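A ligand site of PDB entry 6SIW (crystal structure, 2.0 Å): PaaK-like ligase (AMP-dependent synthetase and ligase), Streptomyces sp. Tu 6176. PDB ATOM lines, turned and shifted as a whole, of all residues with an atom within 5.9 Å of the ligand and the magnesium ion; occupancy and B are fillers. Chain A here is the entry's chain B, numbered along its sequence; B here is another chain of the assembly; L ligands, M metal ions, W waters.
N of Thr 240 sits close to O2 of the ligand (3.0 Å).
An oxygen (O3) of the ligand lies within salt-bridge range of the side-chain amino group (NZ) of Lys 418 of chain B (3.7 Å).
O of Glu 236 is in hydrogen-bond range of N3 of the ligand.
An oxygen (O7) of the ligand lies within hydrogen-bond range of the guanidinium group (NH2) of Arg 323 (3.0 Å).
The side-chain carboxylate (OE2) of Glu 235 sits at hydrogen-bond distance from a nitrogen (N3) of the ligand (2.9 Å).
The side-chain hydroxyl (OG) of Ser 89 sits at hydrogen-bond distance from an oxygen (O3) of the ligand (2.4 Å).
The side-chain carboxylate of Asp 300 is in hydrogen-bond range of an oxygen (O7) of the ligand, at 2.5 Å.
An oxygen (O3) of the ligand lies close to the backbone NH (N) of Ser 89 (3.3 Å).
The backbone NH (N) of Ala 213 is in hydrogen-bond range of a nitrogen (N2) of the ligand (3.1 Å).
O2 of the ligand lies close to OG1 of Thr 240 (3.3 Å).
The side-chain carboxylate (OD2) of Asp 300 is in hydrogen-bond range of the side-chain hydroxyl (OH) of Tyr 237, 2.7 Å away.
The backbone carbonyl oxygen (O) of Leu 298 lies within hydrogen-bond range of the side-chain amino group (NZ) of Lys 63 (2.7 Å).
OG of Ser 88 is in hydrogen-bond range of OE1 of Glu 241.
The side-chain carboxylate of Glu 241 sits at hydrogen-bond distance from the side-chain hydroxyl of Tyr 296.
The backbone NH (N) of Glu 236 lies within hydrogen-bond range of the backbone carbonyl oxygen (O) of Thr 211 (2.9 Å).
N4 of the ligand sits close to O of Glu 214, 3.1 Å away.
Merely in contact with the ligand: Pro 215 (3.3 Å), Gly 238 (3.4 Å), Val 320 (3.5 Å), Tyr 237 (3.6 Å), Ser 239 (3.7 Å), Ser 88 (3.7 Å), Glu 241 (3.8 Å), Leu 298 (3.9 Å) and Met 254 (3.99 Å).
Hydrophobic or aromatic side chains that line the ligand: Tyr 237, Met 254, Leu 298 and Val 320.
The nearest printed residue that does not touch the ligand is Ala 212 (4.2 Å).
Ser 88 touches the magnesium ion (OG to MG, 3.5 Å).
Ser 239 touches the magnesium ion.
Glu 241 touches the magnesium ion.
Of the 26 residues printed, 3 come within 4 Å of the magnesium ion.
The magnesium ion is bound by O2 of the ligand (2.2 Å).
The magnesium ion has one donor atom within binding distance.
Water W3 lies within hydrogen-bond range of O1 of the ligand (2.4 Å) and NZ of Lys 418 of chain B (3.0 Å).
Water W6 lies within hydrogen-bond range of OE2 of Glu 235, N4 of the ligand and N of Leu 216.
Water W4 lies within hydrogen-bond range of the side-chain amino group (NZ) of Lys 63 (2.6 Å) and an oxygen (O6) of the ligand (2.8 Å).
Water W8 bridges O of Ser 89 and O4 of the ligand.
Water W1 lies within hydrogen-bond range of the side-chain hydroxyl (OG1) of Thr 240 (2.8 Å) and an oxygen (O1) of the ligand (3.4 Å).
Water W7 lies within hydrogen-bond range of O of Glu 214 (3.0 Å), OE2 of Glu 235 (3.0 Å) and N3 of the ligand (3.5 Å).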
ATOM      1  N   LYS A  63       6.221  -5.172 -13.239  1.00  0.00           N
ATOM      2  CA  LYS A  63       5.691  -6.517 -13.577  1.00  0.00           C
ATOM      3  C   LYS A  63       4.339  -6.725 -12.904  1.00  0.00           C
ATOM      4  O   LYS A  63       3.415  -7.221 -13.559  1.00  0.00           O
ATOM      5  CB  LYS A  63       6.632  -7.616 -13.082  1.00  0.00           C
ATOM      6  CG  LYS A  63       7.631  -8.140 -14.097  1.00  0.00           C
ATOM      7  CD  LYS A  63       7.652  -9.672 -14.151  1.00  0.00           C
ATOM      8  CE  LYS A  63       8.592 -10.219 -15.204  1.00  0.00           C
ATOM      9  NZ  LYS A  63       9.935  -9.594 -15.102  1.00  0.00           N
ATOM     10  N   SER A  88       3.886 -14.769 -20.624  1.00  0.00           N
ATOM     11  CA  SER A  88       5.321 -14.960 -20.301  1.00  0.00           C
ATOM     12  C   SER A  88       5.487 -16.327 -19.647  1.00  0.00           C
ATOM     13  O   SER A  88       4.506 -16.861 -19.060  1.00  0.00           O
ATOM     14  CB  SER A  88       5.841 -13.853 -19.417  1.00  0.00           C
ATOM     15  OG  SER A  88       5.805 -12.592 -20.084  1.00  0.00           O
ATOM     16  N   SER A  89       6.696 -16.877 -19.715  1.00  0.00           N
ATOM     17  CA  SER A  89       7.177 -18.016 -18.914  1.00  0.00           C
ATOM     18  C   SER A  89       7.126 -17.646 -17.411  1.00  0.00           C
ATOM     19  O   SER A  89       6.721 -16.506 -17.072  1.00  0.00           O
ATOM     20  CB  SER A  89       8.550 -18.443 -19.379  1.00  0.00           C
ATOM     21  OG  SER A  89       9.556 -17.528 -18.939  1.00  0.00           O
ATOM     22  N   GLY A  90       7.502 -18.580 -16.538  1.00  0.00           N
ATOM     23  CA  GLY A  90       7.460 -18.369 -15.075  1.00  0.00           C
ATOM     24  C   GLY A  90       6.157 -18.889 -14.500  1.00  0.00           C
ATOM     25  O   GLY A  90       5.567 -19.815 -15.104  1.00  0.00           O
ATOM     26  N   VAL A 134       4.046 -18.572 -25.112  1.00  0.00           N
ATOM     27  CA  VAL A 134       5.265 -17.723 -25.128  1.00  0.00           C
ATOM     28  C   VAL A 134       5.514 -17.253 -26.564  1.00  0.00           C
ATOM     29  O   VAL A 134       5.038 -17.904 -27.519  1.00  0.00           O
ATOM     30  CB  VAL A 134       6.486 -18.417 -24.497  1.00  0.00           C
ATOM     31  CG1 VAL A 134       6.263 -18.647 -22.997  1.00  0.00           C
ATOM     32  CG2 VAL A 134       6.845 -19.725 -25.190  1.00  0.00           C
ATOM     33  N   THR A 211      20.781 -17.949 -29.442  1.00  0.00           N
ATOM     34  CA  THR A 211      20.405 -18.386 -28.081  1.00  0.00           C
ATOM     35  C   THR A 211      20.006 -17.159 -27.274  1.00  0.00           C
ATOM     36  O   THR A 211      20.378 -16.018 -27.651  1.00  0.00           O
ATOM     37  CB  THR A 211      21.528 -19.233 -27.487  1.00  0.00           C
ATOM     38  OG1 THR A 211      20.981 -20.123 -26.522  1.00  0.00           O
ATOM     39  CG2 THR A 211      22.644 -18.397 -26.905  1.00  0.00           C
ATOM     40  N   ALA A 212      19.291 -17.392 -26.183  1.00  0.00           N
ATOM     41  CA  ALA A 212      18.794 -16.381 -25.227  1.00  0.00           C
ATOM     42  C   ALA A 212      18.216 -17.122 -24.025  1.00  0.00           C
ATOM     43  O   ALA A 212      18.320 -18.353 -23.997  1.00  0.00           O
ATOM     44  CB  ALA A 212      17.746 -15.533 -25.907  1.00  0.00           C
ATOM     45  N   ALA A 213      17.583 -16.397 -23.103  1.00  0.00           N
ATOM     46  CA  ALA A 213      16.624 -16.917 -22.109  1.00  0.00           C
ATOM     47  C   ALA A 213      17.318 -17.286 -20.790  1.00  0.00           C
ATOM     48  O   ALA A 213      16.614 -17.309 -19.799  1.00  0.00           O
ATOM     49  CB  ALA A 213      15.824 -18.075 -22.666  1.00  0.00           C
ATOM     50  N   GLU A 214      18.624 -17.560 -20.784  1.00  0.00           N
ATOM     51  CA  GLU A 214      19.412 -17.818 -19.546  1.00  0.00           C
ATOM     52  C   GLU A 214      20.583 -16.859 -19.460  1.00  0.00           C
ATOM     53  O   GLU A 214      21.151 -16.443 -20.455  1.00  0.00           O
ATOM     54  CB  GLU A 214      20.054 -19.217 -19.507  1.00  0.00           C
ATOM     55  CG  GLU A 214      19.110 -20.378 -19.728  1.00  0.00           C
ATOM     56  CD  GLU A 214      19.832 -21.708 -19.856  1.00  0.00           C
ATOM     57  OE1 GLU A 214      19.341 -22.557 -20.614  1.00  0.00           O
ATOM     58  OE2 GLU A 214      20.839 -21.909 -19.175  1.00  0.00           O
ATOM     59  N   PRO A 215      21.002 -16.523 -18.222  1.00  0.00           N
ATOM     60  CA  PRO A 215      22.319 -15.923 -17.996  1.00  0.00           C
ATOM     61  C   PRO A 215      23.410 -16.828 -18.581  1.00  0.00           C
ATOM     62  O   PRO A 215      23.399 -18.025 -18.347  1.00  0.00           O
ATOM     63  CB  PRO A 215      22.463 -15.848 -16.480  1.00  0.00           C
ATOM     64  CG  PRO A 215      21.068 -16.110 -15.905  1.00  0.00           C
ATOM     65  CD  PRO A 215      20.256 -16.792 -16.980  1.00  0.00           C
ATOM     66  N   LEU A 216      24.260 -16.270 -19.426  1.00  0.00           N
ATOM     67  CA  LEU A 216      25.242 -17.044 -20.217  1.00  0.00           C
ATOM     68  C   LEU A 216      26.594 -16.352 -20.066  1.00  0.00           C
ATOM     69  O   LEU A 216      26.742 -15.234 -20.572  1.00  0.00           O
ATOM     70  CB  LEU A 216      24.788 -17.119 -21.675  1.00  0.00           C
ATOM     71  CG  LEU A 216      25.715 -17.911 -22.599  1.00  0.00           C
ATOM     72  CD1 LEU A 216      25.775 -19.372 -22.180  1.00  0.00           C
ATOM     73  CD2 LEU A 216      25.272 -17.765 -24.046  1.00  0.00           C
ATOM     74  N   GLU A 235      24.032 -14.508 -29.031  1.00  0.00           N
ATOM     75  CA  GLU A 235      23.122 -14.285 -27.900  1.00  0.00           C
ATOM     76  C   GLU A 235      22.239 -13.071 -28.184  1.00  0.00           C
ATOM     77  O   GLU A 235      22.719 -12.074 -28.782  1.00  0.00           O
ATOM     78  CB  GLU A 235      23.940 -14.076 -26.627  1.00  0.00           C
ATOM     79  CG  GLU A 235      23.094 -14.112 -25.374  1.00  0.00           C
ATOM     80  CD  GLU A 235      23.863 -13.838 -24.103  1.00  0.00           C
ATOM     81  OE1 GLU A 235      25.093 -13.572 -24.198  1.00  0.00           O
ATOM     82  OE2 GLU A 235      23.233 -13.883 -23.032  1.00  0.00           O
ATOM     83  N   GLU A 236      21.006 -13.145 -27.738  1.00  0.00           N
ATOM     84  CA  GLU A 236      20.152 -11.946 -27.621  1.00  0.00           C
ATOM     85  C   GLU A 236      19.506 -11.978 -26.247  1.00  0.00           C
ATOM     86  O   GLU A 236      19.566 -13.023 -25.586  1.00  0.00           O
ATOM     87  CB  GLU A 236      19.138 -11.890 -28.775  1.00  0.00           C
ATOM     88  CG  GLU A 236      17.946 -12.816 -28.640  1.00  0.00           C
ATOM     89  CD  GLU A 236      16.796 -12.385 -29.530  1.00  0.00           C
ATOM     90  OE1 GLU A 236      17.035 -12.199 -30.758  1.00  0.00           O
ATOM     91  OE2 GLU A 236      15.682 -12.160 -29.015  1.00  0.00           O
ATOM     92  N   TYR A 237      18.944 -10.845 -25.877  1.00  0.00           N
ATOM     93  CA  TYR A 237      18.269 -10.574 -24.592  1.00  0.00           C
ATOM     94  C   TYR A 237      16.903 -10.008 -24.948  1.00  0.00           C
ATOM     95  O   TYR A 237      16.836  -9.042 -25.733  1.00  0.00           O
ATOM     96  CB  TYR A 237      19.124  -9.608 -23.753  1.00  0.00           C
ATOM     97  CG  TYR A 237      18.476  -9.070 -22.501  1.00  0.00           C
ATOM     98  CD1 TYR A 237      17.680  -9.864 -21.689  1.00  0.00           C
ATOM     99  CD2 TYR A 237      18.712  -7.771 -22.088  1.00  0.00           C
ATOM    100  CE1 TYR A 237      17.109  -9.366 -20.523  1.00  0.00           C
ATOM    101  CE2 TYR A 237      18.148  -7.266 -20.936  1.00  0.00           C
ATOM    102  CZ  TYR A 237      17.339  -8.060 -20.151  1.00  0.00           C
ATOM    103  OH  TYR A 237      16.791  -7.524 -19.010  1.00  0.00           O
ATOM    104  N   GLY A 238      15.846 -10.615 -24.400  1.00  0.00           N
ATOM    105  CA  GLY A 238      14.461 -10.184 -24.618  1.00  0.00           C
ATOM    106  C   GLY A 238      13.527 -10.763 -23.574  1.00  0.00           C
ATOM    107  O   GLY A 238      13.985 -11.369 -22.599  1.00  0.00           O
ATOM    108  N   SER A 239      12.249 -10.535 -23.805  1.00  0.00           N
ATOM    109  CA  SER A 239      11.136 -11.001 -22.951  1.00  0.00           C
ATOM    110  C   SER A 239       9.902 -11.062 -23.844  1.00  0.00           C
ATOM    111  O   SER A 239       9.893 -10.375 -24.883  1.00  0.00           O
ATOM    112  CB  SER A 239      10.944 -10.099 -21.774  1.00  0.00           C
ATOM    113  OG  SER A 239      10.278  -8.905 -22.141  1.00  0.00           O
ATOM    114  N   THR A 240       8.919 -11.846 -23.438  1.00  0.00           N
ATOM    115  CA  THR A 240       7.628 -11.975 -24.145  1.00  0.00           C
ATOM    116  C   THR A 240       7.008 -10.582 -24.269  1.00  0.00           C
ATOM    117  O   THR A 240       6.502 -10.238 -25.360  1.00  0.00           O
ATOM    118  CB  THR A 240       6.752 -13.020 -23.464  1.00  0.00           C
ATOM    119  OG1 THR A 240       7.388 -14.299 -23.561  1.00  0.00           O
ATOM    120  CG2 THR A 240       5.398 -13.113 -24.103  1.00  0.00           C
ATOM    121  N   GLU A 241       7.058  -9.766 -23.213  1.00  0.00           N
ATOM    122  CA  GLU A 241       6.266  -8.521 -23.164  1.00  0.00           C
ATOM    123  C   GLU A 241       7.009  -7.364 -23.823  1.00  0.00           C
ATOM    124  O   GLU A 241       6.352  -6.312 -24.030  1.00  0.00           O
ATOM    125  CB  GLU A 241       5.810  -8.238 -21.722  1.00  0.00           C
ATOM    126  CG  GLU A 241       6.932  -8.114 -20.719  1.00  0.00           C
ATOM    127  CD  GLU A 241       7.348  -9.386 -19.991  1.00  0.00           C
ATOM    128  OE1 GLU A 241       7.097 -10.469 -20.512  1.00  0.00           O
ATOM    129  OE2 GLU A 241       7.959  -9.252 -18.896  1.00  0.00           O
ATOM    130  N   MET A 254      26.478  -7.949 -26.094  1.00  0.00           N
ATOM    131  CA  MET A 254      25.084  -7.594 -26.471  1.00  0.00           C
ATOM    132  C   MET A 254      24.928  -6.071 -26.448  1.00  0.00           C
ATOM    133  O   MET A 254      25.309  -5.430 -25.443  1.00  0.00           O
ATOM    134  CB  MET A 254      24.075  -8.252 -25.533  1.00  0.00           C
ATOM    135  CG  MET A 254      23.969  -9.758 -25.752  1.00  0.00           C
ATOM    136  SD  MET A 254      22.585 -10.508 -24.829  1.00  0.00           S
ATOM    137  CE  MET A 254      23.105 -10.249 -23.126  1.00  0.00           C
ATOM    138  N   TYR A 296       8.688   0.361 -18.347  1.00  0.00           N
ATOM    139  CA  TYR A 296       8.449  -0.996 -17.829  1.00  0.00           C
ATOM    140  C   TYR A 296       9.739  -1.531 -17.208  1.00  0.00           C
ATOM    141  O   TYR A 296      10.744  -1.623 -17.905  1.00  0.00           O
ATOM    142  CB  TYR A 296       7.943  -1.928 -18.944  1.00  0.00           C
ATOM    143  CG  TYR A 296       7.804  -3.365 -18.509  1.00  0.00           C
ATOM    144  CD1 TYR A 296       6.981  -3.716 -17.453  1.00  0.00           C
ATOM    145  CD2 TYR A 296       8.509  -4.371 -19.155  1.00  0.00           C
ATOM    146  CE1 TYR A 296       6.855  -5.037 -17.042  1.00  0.00           C
ATOM    147  CE2 TYR A 296       8.397  -5.697 -18.761  1.00  0.00           C
ATOM    148  CZ  TYR A 296       7.574  -6.026 -17.694  1.00  0.00           C
ATOM    149  OH  TYR A 296       7.471  -7.332 -17.319  1.00  0.00           O
ATOM    150  N   LEU A 298      11.596  -4.567 -16.298  1.00  0.00           N
ATOM    151  CA  LEU A 298      11.758  -6.035 -16.501  1.00  0.00           C
ATOM    152  C   LEU A 298      12.219  -6.682 -15.200  1.00  0.00           C
ATOM    153  O   LEU A 298      12.072  -7.913 -15.088  1.00  0.00           O
ATOM    154  CB  LEU A 298      12.824  -6.341 -17.557  1.00  0.00           C
ATOM    155  CG  LEU A 298      12.310  -6.488 -18.969  1.00  0.00           C
ATOM    156  CD1 LEU A 298      12.093  -5.107 -19.540  1.00  0.00           C
ATOM    157  CD2 LEU A 298      13.272  -7.295 -19.829  1.00  0.00           C
ATOM    158  N   ASP A 300      15.211  -7.317 -14.361  1.00  0.00           N
ATOM    159  CA  ASP A 300      16.517  -8.020 -14.497  1.00  0.00           C
ATOM    160  C   ASP A 300      17.609  -7.105 -13.940  1.00  0.00           C
ATOM    161  O   ASP A 300      17.567  -5.880 -14.204  1.00  0.00           O
ATOM    162  CB  ASP A 300      16.818  -8.454 -15.921  1.00  0.00           C
ATOM    163  CG  ASP A 300      15.893  -9.533 -16.450  1.00  0.00           C
ATOM    164  OD1 ASP A 300      15.631 -10.515 -15.710  1.00  0.00           O
ATOM    165  OD2 ASP A 300      15.445  -9.374 -17.601  1.00  0.00           O
ATOM    166  N   VAL A 320      23.650  -9.107 -18.600  1.00  0.00           N
ATOM    167  CA  VAL A 320      22.451  -9.490 -17.803  1.00  0.00           C
ATOM    168  C   VAL A 320      22.915 -10.434 -16.691  1.00  0.00           C
ATOM    169  O   VAL A 320      23.288 -11.578 -16.989  1.00  0.00           O
ATOM    170  CB  VAL A 320      21.371 -10.115 -18.700  1.00  0.00           C
ATOM    171  CG1 VAL A 320      20.068 -10.301 -17.943  1.00  0.00           C
ATOM    172  CG2 VAL A 320      21.151  -9.303 -19.979  1.00  0.00           C
ATOM    173  N   GLY A 322      21.254 -11.864 -14.296  1.00  0.00           N
ATOM    174  CA  GLY A 322      20.155 -12.632 -13.708  1.00  0.00           C
ATOM    175  C   GLY A 322      19.167 -11.695 -13.030  1.00  0.00           C
ATOM    176  O   GLY A 322      19.392 -10.475 -13.069  1.00  0.00           O
ATOM    177  N   ARG A 323      18.104 -12.229 -12.431  1.00  0.00           N
ATOM    178  CA  ARG A 323      17.079 -11.424 -11.715  1.00  0.00           C
ATOM    179  C   ARG A 323      17.651 -11.003 -10.353  1.00  0.00           C
ATOM    180  O   ARG A 323      17.238  -9.919  -9.893  1.00  0.00           O
ATOM    181  CB  ARG A 323      15.766 -12.184 -11.608  1.00  0.00           C
ATOM    182  CG  ARG A 323      15.015 -12.255 -12.938  1.00  0.00           C
ATOM    183  CD  ARG A 323      13.833 -13.205 -12.904  1.00  0.00           C
ATOM    184  NE  ARG A 323      14.283 -14.593 -12.875  1.00  0.00           N
ATOM    185  CZ  ARG A 323      14.487 -15.369 -13.943  1.00  0.00           C
ATOM    186  NH1 ARG A 323      14.895 -16.612 -13.769  1.00  0.00           N
ATOM    187  NH2 ARG A 323      14.271 -14.920 -15.177  1.00  0.00           N
ATOM    188  N   LYS B 418      12.750 -22.000 -16.978  1.00  0.00           N
ATOM    189  CA  LYS B 418      14.057 -22.035 -17.684  1.00  0.00           C
ATOM    190  C   LYS B 418      14.927 -23.008 -16.891  1.00  0.00           C
ATOM    191  O   LYS B 418      14.577 -23.285 -15.715  1.00  0.00           O
ATOM    192  CB  LYS B 418      14.661 -20.632 -17.755  1.00  0.00           C
ATOM    193  CG  LYS B 418      13.766 -19.561 -18.351  1.00  0.00           C
ATOM    194  CD  LYS B 418      13.487 -19.738 -19.836  1.00  0.00           C
ATOM    195  CE  LYS B 418      12.525 -18.709 -20.391  1.00  0.00           C
ATOM    196  NZ  LYS B 418      12.978 -17.318 -20.134  1.00  0.00           N
HETATM  197  P1  LIG L   1      10.304 -14.674 -21.120  1.00  0.00           P
HETATM  198  O1  LIG L   1      11.082 -14.704 -22.426  1.00  0.00           O
HETATM  199  O2  LIG L   1       9.319 -13.529 -20.986  1.00  0.00           O
HETATM  200  O3  LIG L   1       9.639 -15.994 -20.819  1.00  0.00           O
HETATM  201  O4  LIG L   1      11.517 -14.400 -20.022  1.00  0.00           O
HETATM  202  C1  LIG L   1      12.472 -13.316 -20.271  1.00  0.00           C
HETATM  203  C2  LIG L   1      13.525 -13.247 -19.186  1.00  0.00           C
HETATM  204  O5  LIG L   1      14.578 -14.203 -19.463  1.00  0.00           O
HETATM  205  C3  LIG L   1      14.278 -11.925 -19.057  1.00  0.00           C
HETATM  206  O6  LIG L   1      13.568 -10.925 -18.339  1.00  0.00           O
HETATM  207  C4  LIG L   1      15.528 -12.397 -18.293  1.00  0.00           C
HETATM  208  O7  LIG L   1      15.277 -12.672 -16.927  1.00  0.00           O
HETATM  209  C5  LIG L   1      15.816 -13.706 -19.003  1.00  0.00           C
HETATM  210  N1  LIG L   1      16.720 -13.580 -20.138  1.00  0.00           N
HETATM  211  C6  LIG L   1      16.369 -13.483 -21.463  1.00  0.00           C
HETATM  212  N2  LIG L   1      17.390 -13.393 -22.266  1.00  0.00           N
HETATM  213  C7  LIG L   1      18.496 -13.414 -21.434  1.00  0.00           C
HETATM  214  C8  LIG L   1      19.887 -13.338 -21.687  1.00  0.00           C
HETATM  215  N3  LIG L   1      20.409 -13.239 -22.897  1.00  0.00           N
HETATM  216  N4  LIG L   1      20.726 -13.379 -20.612  1.00  0.00           N
HETATM  217  C9  LIG L   1      20.189 -13.490 -19.388  1.00  0.00           C
HETATM  218  N5  LIG L   1      18.905 -13.583 -19.039  1.00  0.00           N
HETATM  219  C10 LIG L   1      18.096 -13.535 -20.110  1.00  0.00           C
HETATM  220 MG    MG M   1       9.120 -12.301 -19.146  1.00  0.00          MG
HETATM  221  O   HOH W   1       9.173 -15.987 -24.951  1.00  0.00           O
HETATM  222  O   HOH W   2       9.805 -17.829 -23.006  1.00  0.00           O
HETATM  223  O   HOH W   3      13.357 -15.537 -22.524  1.00  0.00           O
HETATM  224  O   HOH W   4      11.056 -10.827 -17.113  1.00  0.00           O
HETATM  225  O   HOH W   5      18.144 -13.604 -16.265  1.00  0.00           O
HETATM  226  O   HOH W   6      23.389 -13.517 -20.608  1.00  0.00           O
HETATM  227  O   HOH W   7      21.652 -16.427 -23.377  1.00  0.00           O
HETATM  228  O   HOH W   8       9.474 -14.606 -17.246  1.00  0.00           O
HETATM  229  O   HOH W   9      11.199 -14.346 -25.343  1.00  0.00           O
